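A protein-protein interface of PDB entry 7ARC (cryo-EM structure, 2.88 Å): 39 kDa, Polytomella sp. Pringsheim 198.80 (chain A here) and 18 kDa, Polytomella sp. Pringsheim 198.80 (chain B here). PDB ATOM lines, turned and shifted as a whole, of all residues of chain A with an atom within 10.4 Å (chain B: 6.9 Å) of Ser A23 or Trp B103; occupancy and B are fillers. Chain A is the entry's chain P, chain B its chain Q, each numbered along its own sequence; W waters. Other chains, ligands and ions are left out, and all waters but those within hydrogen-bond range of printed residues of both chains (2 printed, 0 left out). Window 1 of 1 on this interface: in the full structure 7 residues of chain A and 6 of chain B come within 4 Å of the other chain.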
ATOM      1  N   ALA A  14      12.314  -4.024  20.925  1.00  0.00           N
ATOM      2  CA  ALA A  14      12.353  -4.971  22.036  1.00  0.00           C
ATOM      3  C   ALA A  14      10.998  -5.637  22.244  1.00  0.00           C
ATOM      4  O   ALA A  14      10.892  -6.869  22.258  1.00  0.00           O
ATOM      5  CB  ALA A  14      12.802  -4.257  23.311  1.00  0.00           C
ATOM      6  N   VAL A  15       9.948  -4.834  22.418  1.00  0.00           N
ATOM      7  CA  VAL A  15       8.641  -5.370  22.792  1.00  0.00           C
ATOM      8  C   VAL A  15       7.984  -6.126  21.637  1.00  0.00           C
ATOM      9  O   VAL A  15       7.351  -7.165  21.853  1.00  0.00           O
ATOM     10  CB  VAL A  15       7.748  -4.239  23.332  1.00  0.00           C
ATOM     11  CG1 VAL A  15       8.358  -3.658  24.587  1.00  0.00           C
ATOM     12  CG2 VAL A  15       7.621  -3.143  22.306  1.00  0.00           C
ATOM     13  N   ARG A  16       8.096  -5.621  20.407  1.00  0.00           N
ATOM     14  CA  ARG A  16       7.378  -6.221  19.286  1.00  0.00           C
ATOM     15  C   ARG A  16       7.798  -7.674  19.089  1.00  0.00           C
ATOM     16  O   ARG A  16       8.970  -8.025  19.252  1.00  0.00           O
ATOM     17  CB  ARG A  16       7.635  -5.459  17.986  1.00  0.00           C
ATOM     18  CG  ARG A  16       9.070  -5.547  17.530  1.00  0.00           C
ATOM     19  CD  ARG A  16       9.370  -4.763  16.280  1.00  0.00           C
ATOM     20  NE  ARG A  16      10.776  -4.933  15.940  1.00  0.00           N
ATOM     21  CZ  ARG A  16      11.369  -4.394  14.887  1.00  0.00           C
ATOM     22  NH1 ARG A  16      10.702  -3.651  14.027  1.00  0.00           N
ATOM     23  NH2 ARG A  16      12.665  -4.617  14.687  1.00  0.00           N
ATOM     24  N   ASN A  17       6.830  -8.526  18.756  1.00  0.00           N
ATOM     25  CA  ASN A  17       7.142  -9.904  18.406  1.00  0.00           C
ATOM     26  C   ASN A  17       5.908 -10.541  17.784  1.00  0.00           C
ATOM     27  O   ASN A  17       4.785 -10.254  18.198  1.00  0.00           O
ATOM     28  CB  ASN A  17       7.608 -10.700  19.633  1.00  0.00           C
ATOM     29  CG  ASN A  17       8.149 -12.069  19.270  1.00  0.00           C
ATOM     30  OD1 ASN A  17       8.151 -12.463  18.105  1.00  0.00           O
ATOM     31  ND2 ASN A  17       8.671 -12.774  20.262  1.00  0.00           N
ATOM     32  N   GLY A  18       6.130 -11.400  16.792  1.00  0.00           N
ATOM     33  CA  GLY A  18       5.054 -12.035  16.069  1.00  0.00           C
ATOM     34  C   GLY A  18       4.946 -11.535  14.644  1.00  0.00           C
ATOM     35  O   GLY A  18       5.647 -10.605  14.233  1.00  0.00           O
ATOM     36  N   PRO A  19       4.050 -12.138  13.858  1.00  0.00           N
ATOM     37  CA  PRO A  19       3.940 -11.765  12.439  1.00  0.00           C
ATOM     38  C   PRO A  19       3.342 -10.392  12.189  1.00  0.00           C
ATOM     39  O   PRO A  19       3.436  -9.905  11.056  1.00  0.00           O
ATOM     40  CB  PRO A  19       3.043 -12.869  11.857  1.00  0.00           C
ATOM     41  CG  PRO A  19       3.082 -13.958  12.870  1.00  0.00           C
ATOM     42  CD  PRO A  19       3.165 -13.264  14.174  1.00  0.00           C
ATOM     43  N   GLY A  20       2.729  -9.754  13.179  1.00  0.00           N
ATOM     44  CA  GLY A  20       2.013  -8.521  12.936  1.00  0.00           C
ATOM     45  C   GLY A  20       0.508  -8.627  12.860  1.00  0.00           C
ATOM     46  O   GLY A  20      -0.133  -7.676  12.402  1.00  0.00           O
ATOM     47  N   GLY A  21      -0.075  -9.742  13.281  1.00  0.00           N
ATOM     48  CA  GLY A  21      -1.499  -9.949  13.200  1.00  0.00           C
ATOM     49  C   GLY A  21      -2.220  -9.610  14.488  1.00  0.00           C
ATOM     50  O   GLY A  21      -1.704  -8.901  15.358  1.00  0.00           O
ATOM     51  N   ARG A  22      -3.443 -10.126  14.602  1.00  0.00           N
ATOM     52  CA  ARG A  22      -4.283  -9.851  15.764  1.00  0.00           C
ATOM     53  C   ARG A  22      -3.642 -10.356  17.051  1.00  0.00           C
ATOM     54  O   ARG A  22      -3.628  -9.654  18.068  1.00  0.00           O
ATOM     55  CB  ARG A  22      -5.668 -10.460  15.548  1.00  0.00           C
ATOM     56  CG  ARG A  22      -6.668 -10.165  16.642  1.00  0.00           C
ATOM     57  CD  ARG A  22      -8.032 -10.733  16.288  1.00  0.00           C
ATOM     58  NE  ARG A  22      -9.015 -10.495  17.338  1.00  0.00           N
ATOM     59  CZ  ARG A  22     -10.284 -10.870  17.270  1.00  0.00           C
ATOM     60  NH1 ARG A  22     -10.767 -11.479  16.202  1.00  0.00           N
ATOM     61  NH2 ARG A  22     -11.091 -10.614  18.293  1.00  0.00           N
ATOM     62  N   SER A  23      -3.113 -11.576  17.029  1.00  0.00           N
ATOM     63  CA  SER A  23      -2.532 -12.205  18.208  1.00  0.00           C
ATOM     64  C   SER A  23      -1.071 -11.836  18.425  1.00  0.00           C
ATOM     65  O   SER A  23      -0.499 -12.211  19.453  1.00  0.00           O
ATOM     66  CB  SER A  23      -2.662 -13.727  18.109  1.00  0.00           C
ATOM     67  OG  SER A  23      -4.021 -14.121  18.112  1.00  0.00           O
ATOM     68  N   SER A  24      -0.457 -11.126  17.485  1.00  0.00           N
ATOM     69  CA  SER A  24       0.918 -10.673  17.621  1.00  0.00           C
ATOM     70  C   SER A  24       1.011  -9.520  18.617  1.00  0.00           C
ATOM     71  O   SER A  24       0.009  -8.947  19.049  1.00  0.00           O
ATOM     72  CB  SER A  24       1.456 -10.217  16.272  1.00  0.00           C
ATOM     73  OG  SER A  24       1.294 -11.234  15.311  1.00  0.00           O
ATOM     74  N   ILE A  25       2.242  -9.189  18.994  1.00  0.00           N
ATOM     75  CA  ILE A  25       2.516  -8.100  19.924  1.00  0.00           C
ATOM     76  C   ILE A  25       3.084  -6.933  19.133  1.00  0.00           C
ATOM     77  O   ILE A  25       4.156  -7.043  18.528  1.00  0.00           O
ATOM     78  CB  ILE A  25       3.489  -8.517  21.036  1.00  0.00           C
ATOM     79  CG1 ILE A  25       2.991  -9.760  21.766  1.00  0.00           C
ATOM     80  CG2 ILE A  25       3.697  -7.376  22.013  1.00  0.00           C
ATOM     81  CD1 ILE A  25       3.991 -10.299  22.754  1.00  0.00           C
ATOM     82  N   GLY A  26       2.366  -5.818  19.138  1.00  0.00           N
ATOM     83  CA  GLY A  26       2.878  -4.550  18.645  1.00  0.00           C
ATOM     84  C   GLY A  26       3.152  -3.641  19.830  1.00  0.00           C
ATOM     85  O   GLY A  26       2.400  -3.641  20.808  1.00  0.00           O
ATOM     86  N   ILE A  47      -5.142   0.139  14.291  1.00  0.00           N
ATOM     87  CA  ILE A  47      -4.121  -0.029  15.321  1.00  0.00           C
ATOM     88  C   ILE A  47      -4.258  -1.384  16.007  1.00  0.00           C
ATOM     89  O   ILE A  47      -3.262  -2.079  16.235  1.00  0.00           O
ATOM     90  CB  ILE A  47      -4.182   1.131  16.331  1.00  0.00           C
ATOM     91  CG1 ILE A  47      -3.963   2.463  15.618  1.00  0.00           C
ATOM     92  CG2 ILE A  47      -3.151   0.940  17.424  1.00  0.00           C
ATOM     93  CD1 ILE A  47      -4.203   3.664  16.490  1.00  0.00           C
ATOM     94  N   SER A  48      -5.485  -1.797  16.328  1.00  0.00           N
ATOM     95  CA  SER A  48      -5.687  -3.023  17.087  1.00  0.00           C
ATOM     96  C   SER A  48      -5.524  -4.271  16.229  1.00  0.00           C
ATOM     97  O   SER A  48      -5.170  -5.333  16.749  1.00  0.00           O
ATOM     98  CB  SER A  48      -7.068  -3.006  17.736  1.00  0.00           C
ATOM     99  OG  SER A  48      -7.302  -4.197  18.458  1.00  0.00           O
ATOM    100  N   LYS A  49      -5.796  -4.164  14.927  1.00  0.00           N
ATOM    101  CA  LYS A  49      -5.664  -5.285  14.008  1.00  0.00           C
ATOM    102  C   LYS A  49      -4.254  -5.856  14.005  1.00  0.00           C
ATOM    103  O   LYS A  49      -4.073  -7.064  13.818  1.00  0.00           O
ATOM    104  CB  LYS A  49      -6.068  -4.816  12.614  1.00  0.00           C
ATOM    105  CG  LYS A  49      -6.036  -5.847  11.528  1.00  0.00           C
ATOM    106  CD  LYS A  49      -6.588  -5.241  10.257  1.00  0.00           C
ATOM    107  CE  LYS A  49      -5.600  -4.259   9.662  1.00  0.00           C
ATOM    108  NZ  LYS A  49      -6.060  -3.731   8.353  1.00  0.00           N
ATOM    109  N   ARG A  50      -3.250  -5.010  14.213  1.00  0.00           N
ATOM    110  CA  ARG A  50      -1.854  -5.405  14.146  1.00  0.00           C
ATOM    111  C   ARG A  50      -1.295  -5.813  15.501  1.00  0.00           C
ATOM    112  O   ARG A  50      -0.075  -5.786  15.695  1.00  0.00           O
ATOM    113  CB  ARG A  50      -1.026  -4.274  13.538  1.00  0.00           C
ATOM    114  CG  ARG A  50      -1.592  -3.788  12.221  1.00  0.00           C
ATOM    115  CD  ARG A  50      -0.848  -2.592  11.681  1.00  0.00           C
ATOM    116  NE  ARG A  50      -0.927  -2.545  10.227  1.00  0.00           N
ATOM    117  CZ  ARG A  50      -1.935  -2.014   9.550  1.00  0.00           C
ATOM    118  NH1 ARG A  50      -2.973  -1.478  10.167  1.00  0.00           N
ATOM    119  NH2 ARG A  50      -1.904  -2.028   8.222  1.00  0.00           N
ATOM    120  N   GLY A  51      -2.159  -6.200  16.434  1.00  0.00           N
ATOM    121  CA  GLY A  51      -1.729  -6.693  17.722  1.00  0.00           C
ATOM    122  C   GLY A  51      -1.445  -5.643  18.767  1.00  0.00           C
ATOM    123  O   GLY A  51      -0.922  -5.983  19.833  1.00  0.00           O
ATOM    124  N   ASN A  52      -1.766  -4.384  18.505  1.00  0.00           N
ATOM    125  CA  ASN A  52      -1.501  -3.318  19.455  1.00  0.00           C
ATOM    126  C   ASN A  52      -2.680  -3.161  20.409  1.00  0.00           C
ATOM    127  O   ASN A  52      -3.778  -3.661  20.165  1.00  0.00           O
ATOM    128  CB  ASN A  52      -1.234  -2.005  18.725  1.00  0.00           C
ATOM    129  CG  ASN A  52      -0.206  -2.150  17.629  1.00  0.00           C
ATOM    130  OD1 ASN A  52       0.993  -2.066  17.872  1.00  0.00           O
ATOM    131  ND2 ASN A  52      -0.672  -2.364  16.408  1.00  0.00           N
ATOM    132  N   GLN A  53      -2.435  -2.461  21.511  1.00  0.00           N
ATOM    133  CA  GLN A  53      -3.445  -2.240  22.535  1.00  0.00           C
ATOM    134  C   GLN A  53      -3.988  -0.822  22.415  1.00  0.00           C
ATOM    135  O   GLN A  53      -3.215   0.138  22.360  1.00  0.00           O
ATOM    136  CB  GLN A  53      -2.867  -2.481  23.929  1.00  0.00           C
ATOM    137  CG  GLN A  53      -3.763  -2.028  25.059  1.00  0.00           C
ATOM    138  CD  GLN A  53      -3.329  -2.590  26.390  1.00  0.00           C
ATOM    139  OE1 GLN A  53      -2.219  -2.338  26.850  1.00  0.00           O
ATOM    140  NE2 GLN A  53      -4.202  -3.367  27.015  1.00  0.00           N
ATOM    141  N   GLN A  70     -15.071  -6.259  19.324  1.00  0.00           N
ATOM    142  CA  GLN A  70     -14.579  -7.282  18.409  1.00  0.00           C
ATOM    143  C   GLN A  70     -13.226  -6.932  17.797  1.00  0.00           C
ATOM    144  O   GLN A  70     -12.556  -7.827  17.273  1.00  0.00           O
ATOM    145  CB  GLN A  70     -15.633  -7.511  17.316  1.00  0.00           C
ATOM    146  CG  GLN A  70     -15.391  -8.681  16.371  1.00  0.00           C
ATOM    147  CD  GLN A  70     -14.508  -8.336  15.191  1.00  0.00           C
ATOM    148  OE1 GLN A  70     -14.483  -7.197  14.731  1.00  0.00           O
ATOM    149  NE2 GLN A  70     -13.775  -9.323  14.694  1.00  0.00           N
ATOM    150  N   MET A  71     -12.789  -5.673  17.891  1.00  0.00           N
ATOM    151  CA  MET A  71     -11.670  -5.206  17.076  1.00  0.00           C
ATOM    152  C   MET A  71     -10.381  -5.958  17.378  1.00  0.00           C
ATOM    153  O   MET A  71      -9.577  -6.208  16.474  1.00  0.00           O
ATOM    154  CB  MET A  71     -11.452  -3.710  17.289  1.00  0.00           C
ATOM    155  CG  MET A  71     -12.606  -2.841  16.874  1.00  0.00           C
ATOM    156  SD  MET A  71     -12.674  -2.429  15.135  1.00  0.00           S
ATOM    157  CE  MET A  71     -13.934  -1.162  15.171  1.00  0.00           C
ATOM    158  N   GLY A  72     -10.158  -6.326  18.642  1.00  0.00           N
ATOM    159  CA  GLY A  72      -8.881  -6.856  19.059  1.00  0.00           C
ATOM    160  C   GLY A  72      -9.032  -8.098  19.918  1.00  0.00           C
ATOM    161  O   GLY A  72     -10.132  -8.481  20.320  1.00  0.00           O
ATOM    162  N   ASP A  73      -7.888  -8.711  20.202  1.00  0.00           N
ATOM    163  CA  ASP A  73      -7.826  -9.933  20.992  1.00  0.00           C
ATOM    164  C   ASP A  73      -8.059  -9.572  22.462  1.00  0.00           C
ATOM    165  O   ASP A  73      -8.371  -8.430  22.803  1.00  0.00           O
ATOM    166  CB  ASP A  73      -6.495 -10.638  20.736  1.00  0.00           C
ATOM    167  CG  ASP A  73      -6.430 -12.029  21.347  1.00  0.00           C
ATOM    168  OD1 ASP A  73      -7.409 -12.444  22.001  1.00  0.00           O
ATOM    169  OD2 ASP A  73      -5.396 -12.708  21.172  1.00  0.00           O
ATOM    170  N   LEU A  74      -7.916 -10.551  23.354  1.00  0.00           N
ATOM    171  CA  LEU A  74      -8.224 -10.347  24.763  1.00  0.00           C
ATOM    172  C   LEU A  74      -7.314  -9.298  25.387  1.00  0.00           C
ATOM    173  O   LEU A  74      -6.087  -9.386  25.298  1.00  0.00           O
ATOM    174  CB  LEU A  74      -8.097 -11.666  25.520  1.00  0.00           C
ATOM    175  CG  LEU A  74      -9.123 -12.722  25.124  1.00  0.00           C
ATOM    176  CD1 LEU A  74      -8.847 -14.041  25.816  1.00  0.00           C
ATOM    177  CD2 LEU A  74     -10.501 -12.209  25.467  1.00  0.00           C
ATOM    178  N   GLY A  75      -7.928  -8.305  26.027  1.00  0.00           N
ATOM    179  CA  GLY A  75      -7.201  -7.277  26.735  1.00  0.00           C
ATOM    180  C   GLY A  75      -6.587  -6.201  25.870  1.00  0.00           C
ATOM    181  O   GLY A  75      -5.882  -5.333  26.400  1.00  0.00           O
ATOM    182  N   GLN A  76      -6.837  -6.216  24.563  1.00  0.00           N
ATOM    183  CA  GLN A  76      -6.208  -5.260  23.664  1.00  0.00           C
ATOM    184  C   GLN A  76      -7.025  -3.985  23.508  1.00  0.00           C
ATOM    185  O   GLN A  76      -6.454  -2.893  23.426  1.00  0.00           O
ATOM    186  CB  GLN A  76      -5.980  -5.903  22.295  1.00  0.00           C
ATOM    187  CG  GLN A  76      -5.018  -7.076  22.325  1.00  0.00           C
ATOM    188  CD  GLN A  76      -3.608  -6.669  22.687  1.00  0.00           C
ATOM    189  OE1 GLN A  76      -3.123  -5.622  22.266  1.00  0.00           O
ATOM    190  NE2 GLN A  76      -2.943  -7.494  23.482  1.00  0.00           N
ATOM    191  N   SER B 101       9.651 -18.625  15.439  1.00  0.00           N
ATOM    192  CA  SER B 101       9.454 -17.664  16.516  1.00  0.00           C
ATOM    193  C   SER B 101       8.322 -18.070  17.454  1.00  0.00           C
ATOM    194  O   SER B 101       7.304 -18.623  17.033  1.00  0.00           O
ATOM    195  CB  SER B 101       9.174 -16.278  15.940  1.00  0.00           C
ATOM    196  OG  SER B 101       7.936 -16.253  15.255  1.00  0.00           O
ATOM    197  N   LYS B 102       8.518 -17.783  18.737  1.00  0.00           N
ATOM    198  CA  LYS B 102       7.538 -18.003  19.788  1.00  0.00           C
ATOM    199  C   LYS B 102       7.578 -16.806  20.722  1.00  0.00           C
ATOM    200  O   LYS B 102       8.655 -16.287  21.019  1.00  0.00           O
ATOM    201  CB  LYS B 102       7.819 -19.278  20.585  1.00  0.00           C
ATOM    202  CG  LYS B 102       7.691 -20.562  19.806  1.00  0.00           C
ATOM    203  CD  LYS B 102       7.979 -21.749  20.700  1.00  0.00           C
ATOM    204  CE  LYS B 102       7.779 -23.051  19.961  1.00  0.00           C
ATOM    205  NZ  LYS B 102       8.783 -23.225  18.880  1.00  0.00           N
ATOM    206  N   TRP B 103       6.411 -16.363  21.180  1.00  0.00           N
ATOM    207  CA  TRP B 103       6.346 -15.227  22.083  1.00  0.00           C
ATOM    208  C   TRP B 103       5.349 -15.536  23.188  1.00  0.00           C
ATOM    209  O   TRP B 103       4.758 -16.617  23.238  1.00  0.00           O
ATOM    210  CB  TRP B 103       5.989 -13.928  21.349  1.00  0.00           C
ATOM    211  CG  TRP B 103       4.677 -13.914  20.643  1.00  0.00           C
ATOM    212  CD1 TRP B 103       3.525 -13.340  21.077  1.00  0.00           C
ATOM    213  CD2 TRP B 103       4.390 -14.470  19.358  1.00  0.00           C
ATOM    214  NE1 TRP B 103       2.532 -13.515  20.152  1.00  0.00           N
ATOM    215  CE2 TRP B 103       3.038 -14.206  19.084  1.00  0.00           C
ATOM    216  CE3 TRP B 103       5.143 -15.172  18.415  1.00  0.00           C
ATOM    217  CZ2 TRP B 103       2.421 -14.620  17.912  1.00  0.00           C
ATOM    218  CZ3 TRP B 103       4.530 -15.579  17.253  1.00  0.00           C
ATOM    219  CH2 TRP B 103       3.184 -15.305  17.011  1.00  0.00           C
ATOM    220  N   GLU B 104       5.174 -14.575  24.086  1.00  0.00           N
ATOM    221  CA  GLU B 104       4.337 -14.734  25.264  1.00  0.00           C
ATOM    222  C   GLU B 104       3.092 -13.880  25.106  1.00  0.00           C
ATOM    223  O   GLU B 104       3.183 -12.709  24.725  1.00  0.00           O
ATOM    224  CB  GLU B 104       5.091 -14.341  26.534  1.00  0.00           C
ATOM    225  CG  GLU B 104       6.457 -14.984  26.658  1.00  0.00           C
ATOM    226  CD  GLU B 104       6.382 -16.436  27.073  1.00  0.00           C
ATOM    227  OE1 GLU B 104       7.117 -17.260  26.490  1.00  0.00           O
ATOM    228  OE2 GLU B 104       5.592 -16.755  27.985  1.00  0.00           O
ATOM    229  N   ASN B 105       1.941 -14.469  25.386  1.00  0.00           N
ATOM    230  CA  ASN B 105       0.695 -13.724  25.343  1.00  0.00           C
ATOM    231  C   ASN B 105       0.760 -12.563  26.329  1.00  0.00           C
ATOM    232  O   ASN B 105       1.046 -12.779  27.513  1.00  0.00           O
ATOM    233  CB  ASN B 105      -0.477 -14.643  25.678  1.00  0.00           C
ATOM    234  CG  ASN B 105      -1.814 -13.995  25.427  1.00  0.00           C
ATOM    235  OD1 ASN B 105      -1.973 -13.221  24.487  1.00  0.00           O
ATOM    236  ND2 ASN B 105      -2.790 -14.314  26.264  1.00  0.00           N
ATOM    237  N   PRO B 106       0.524 -11.327  25.885  1.00  0.00           N
ATOM    238  CA  PRO B 106       0.602 -10.190  26.812  1.00  0.00           C
ATOM    239  C   PRO B 106      -0.352 -10.286  27.989  1.00  0.00           C
ATOM    240  O   PRO B 106      -0.016  -9.808  29.078  1.00  0.00           O
ATOM    241  CB  PRO B 106       0.285  -8.983  25.915  1.00  0.00           C
ATOM    242  CG  PRO B 106      -0.384  -9.548  24.715  1.00  0.00           C
ATOM    243  CD  PRO B 106       0.200 -10.904  24.514  1.00  0.00           C
ATOM    244  N   GLY B 109       0.501 -14.562  29.477  1.00  0.00           N
ATOM    245  CA  GLY B 109       1.823 -15.152  29.437  1.00  0.00           C
ATOM    246  C   GLY B 109       1.896 -16.509  28.781  1.00  0.00           C
ATOM    247  O   GLY B 109       2.902 -17.203  28.935  1.00  0.00           O
ATOM    248  N   TRP B 110       0.857 -16.909  28.059  1.00  0.00           N
ATOM    249  CA  TRP B 110       0.871 -18.158  27.320  1.00  0.00           C
ATOM    250  C   TRP B 110       1.839 -18.075  26.147  1.00  0.00           C
ATOM    251  O   TRP B 110       2.107 -16.998  25.610  1.00  0.00           O
ATOM    252  CB  TRP B 110      -0.531 -18.474  26.813  1.00  0.00           C
ATOM    253  CG  TRP B 110      -1.471 -18.820  27.904  1.00  0.00           C
ATOM    254  CD1 TRP B 110      -1.151 -19.285  29.141  1.00  0.00           C
ATOM    255  CD2 TRP B 110      -2.893 -18.692  27.877  1.00  0.00           C
ATOM    256  NE1 TRP B 110      -2.287 -19.473  29.883  1.00  0.00           N
ATOM    257  CE2 TRP B 110      -3.372 -19.115  29.129  1.00  0.00           C
ATOM    258  CE3 TRP B 110      -3.809 -18.267  26.912  1.00  0.00           C
ATOM    259  CZ2 TRP B 110      -4.725 -19.129  29.441  1.00  0.00           C
ATOM    260  CZ3 TRP B 110      -5.150 -18.281  27.224  1.00  0.00           C
ATOM    261  CH2 TRP B 110      -5.597 -18.709  28.476  1.00  0.00           C
ATOM    262  N   THR B 111       2.371 -19.227  25.752  1.00  0.00           N
ATOM    263  CA  THR B 111       3.298 -19.294  24.628  1.00  0.00           C
ATOM    264  C   THR B 111       2.513 -19.254  23.323  1.00  0.00           C
ATOM    265  O   THR B 111       1.748 -20.173  23.021  1.00  0.00           O
ATOM    266  CB  THR B 111       4.155 -20.552  24.710  1.00  0.00           C
ATOM    267  OG1 THR B 111       4.609 -20.733  26.056  1.00  0.00           O
ATOM    268  CG2 THR B 111       5.355 -20.430  23.792  1.00  0.00           C
ATOM    269  N   SER B 112       2.701 -18.192  22.550  1.00  0.00           N
ATOM    270  CA  SER B 112       2.003 -18.000  21.290  1.00  0.00           C
ATOM    271  C   SER B 112       2.927 -18.333  20.127  1.00  0.00           C
ATOM    272  O   SER B 112       4.147 -18.189  20.222  1.00  0.00           O
ATOM    273  CB  SER B 112       1.502 -16.562  21.161  1.00  0.00           C
ATOM    274  OG  SER B 112       0.542 -16.267  22.156  1.00  0.00           O
ATOM    275  N   THR B 113       2.336 -18.790  19.025  1.00  0.00           N
ATOM    276  CA  THR B 113       3.122 -19.199  17.872  1.00  0.00           C
ATOM    277  C   THR B 113       2.339 -18.910  16.602  1.00  0.00           C
ATOM    278  O   THR B 113       1.118 -18.742  16.625  1.00  0.00           O
ATOM    279  CB  THR B 113       3.491 -20.685  17.932  1.00  0.00           C
ATOM    280  OG1 THR B 113       4.405 -20.993  16.875  1.00  0.00           O
ATOM    281  CG2 THR B 113       2.251 -21.542  17.768  1.00  0.00           C
ATOM    282  N   ALA B 114       3.066 -18.837  15.488  1.00  0.00           N
ATOM    283  CA  ALA B 114       2.460 -18.735  14.167  1.00  0.00           C
ATOM    284  C   ALA B 114       2.908 -19.850  13.234  1.00  0.00           C
ATOM    285  O   ALA B 114       2.681 -19.758  12.023  1.00  0.00           O
ATOM    286  CB  ALA B 114       2.774 -17.378  13.539  1.00  0.00           C
ATOM    287  N   ASP B 115       3.546 -20.894  13.760  1.00  0.00           N
ATOM    288  CA  ASP B 115       4.070 -21.972  12.935  1.00  0.00           C
ATOM    289  C   ASP B 115       3.006 -23.049  12.782  1.00  0.00           C
ATOM    290  O   ASP B 115       2.653 -23.698  13.778  1.00  0.00           O
ATOM    291  CB  ASP B 115       5.329 -22.553  13.560  1.00  0.00           C
ATOM    292  CG  ASP B 115       6.077 -23.472  12.619  1.00  0.00           C
ATOM    293  OD1 ASP B 115       5.724 -23.523  11.423  1.00  0.00           O
ATOM    294  OD2 ASP B 115       7.023 -24.146  13.078  1.00  0.00           O
HETATM  295  O   HOH W   1      -0.605 -13.410  21.885  1.00  0.00           O
HETATM  296  O   HOH W   2      -3.981 -10.424  24.447  1.00  0.00           O
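The backbone carbonyl oxygen (O) of Ser A23 sits at hydrogen-bond distance from the indole nitrogen (NE1) of Trp B103 (3.4 Å).
Hydrophobic or aromatic side chains of chain B that line the printed part of chain A: Trp B103, Pro B106 and Ala B114. Hydrophobic or aromatic side chains of chain A that line the printed part of chain B: Pro A19 and Ile A25.
Water W2 lies within hydrogen-bond range of O of Leu A74, NE2 of Gln A76 and OD1 of Asn B105. Water W1 lies within hydrogen-bond range of the backbone carbonyl oxygen of Ser A23 (2.7 Å), the side-chain amide oxygen of Asn B105 (2.9 Å) and the side-chain hydroxyl of Ser B112 (3.1 Å).
Of the printed residues of chain B, Ser A23 touches Trp B103 (3.4 Å). Of chain A, only Asn A17 (3.1 Å), Gly A18 (3.8 Å), Pro A19 (3.5 Å), Ser A23 (3.4 Å) and Ile A25 (3.5 Å) come within 4 Å of Trp B103. No residue of chain A comes within 4 Å of Ser B101. Glu B104 touches just one residue of chain A: Ile A25. No residue of chain A comes within 4 Å of Thr B111. Printed residues of chain B within 4 Å of Gln A76: Pro B106 (3.5 Å). Of the printed residues of chain A, Ala B114 touches Pro A19 (3.5 Å). Of the printed residues of chain A, Lys B102 touches Asn A17 (3.6 Å). Of the printed residues of chain B, Ile A25 touches Trp B103 (3.5 Å) and Glu B104 (3.2 Å). Of the printed residues of chain B, Gly A18 touches Trp B103 (3.8 Å). Asn A52 touches none of the printed residues of chain B. Trp B110 touches none of the printed residues of chain A. The nearest printed residue of chain B that does not touch Asn A17 is Ser B101 (4.5 Å).
Asn A17 touches Lys B102. Asn A17 touches Trp B103 (ND2 to CB, 3.1 Å). CA of Gly A18 touches CZ3 of Trp B103, at 3.8 Å. CH2 of Trp B103 touches CD of Pro A19, 3.5 Å away. Pro A19 touches Ala B114. Ile A25 touches Trp B103. Ile A25 touches Glu B104. NE2 of Gln A76 touches CG of Pro B106, 3.5 Å away.
The side-chain amide oxygen of Gln A76 lies close to the backbone carbonyl oxygen of Gly A51 (3.3 Å). N of Gln A53 sits at hydrogen-bond distance from OE1 of Gln A76. The backbone carbonyl oxygen (O) of Trp B103 is in hydrogen-bond range of the backbone NH (N) of Ser B112. O of Asn A52 sits close to OE1 of Gln A76 (2.9 Å). O of Asn A17 lies within hydrogen-bond range of N of Ile A25, 2.9 Å away.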
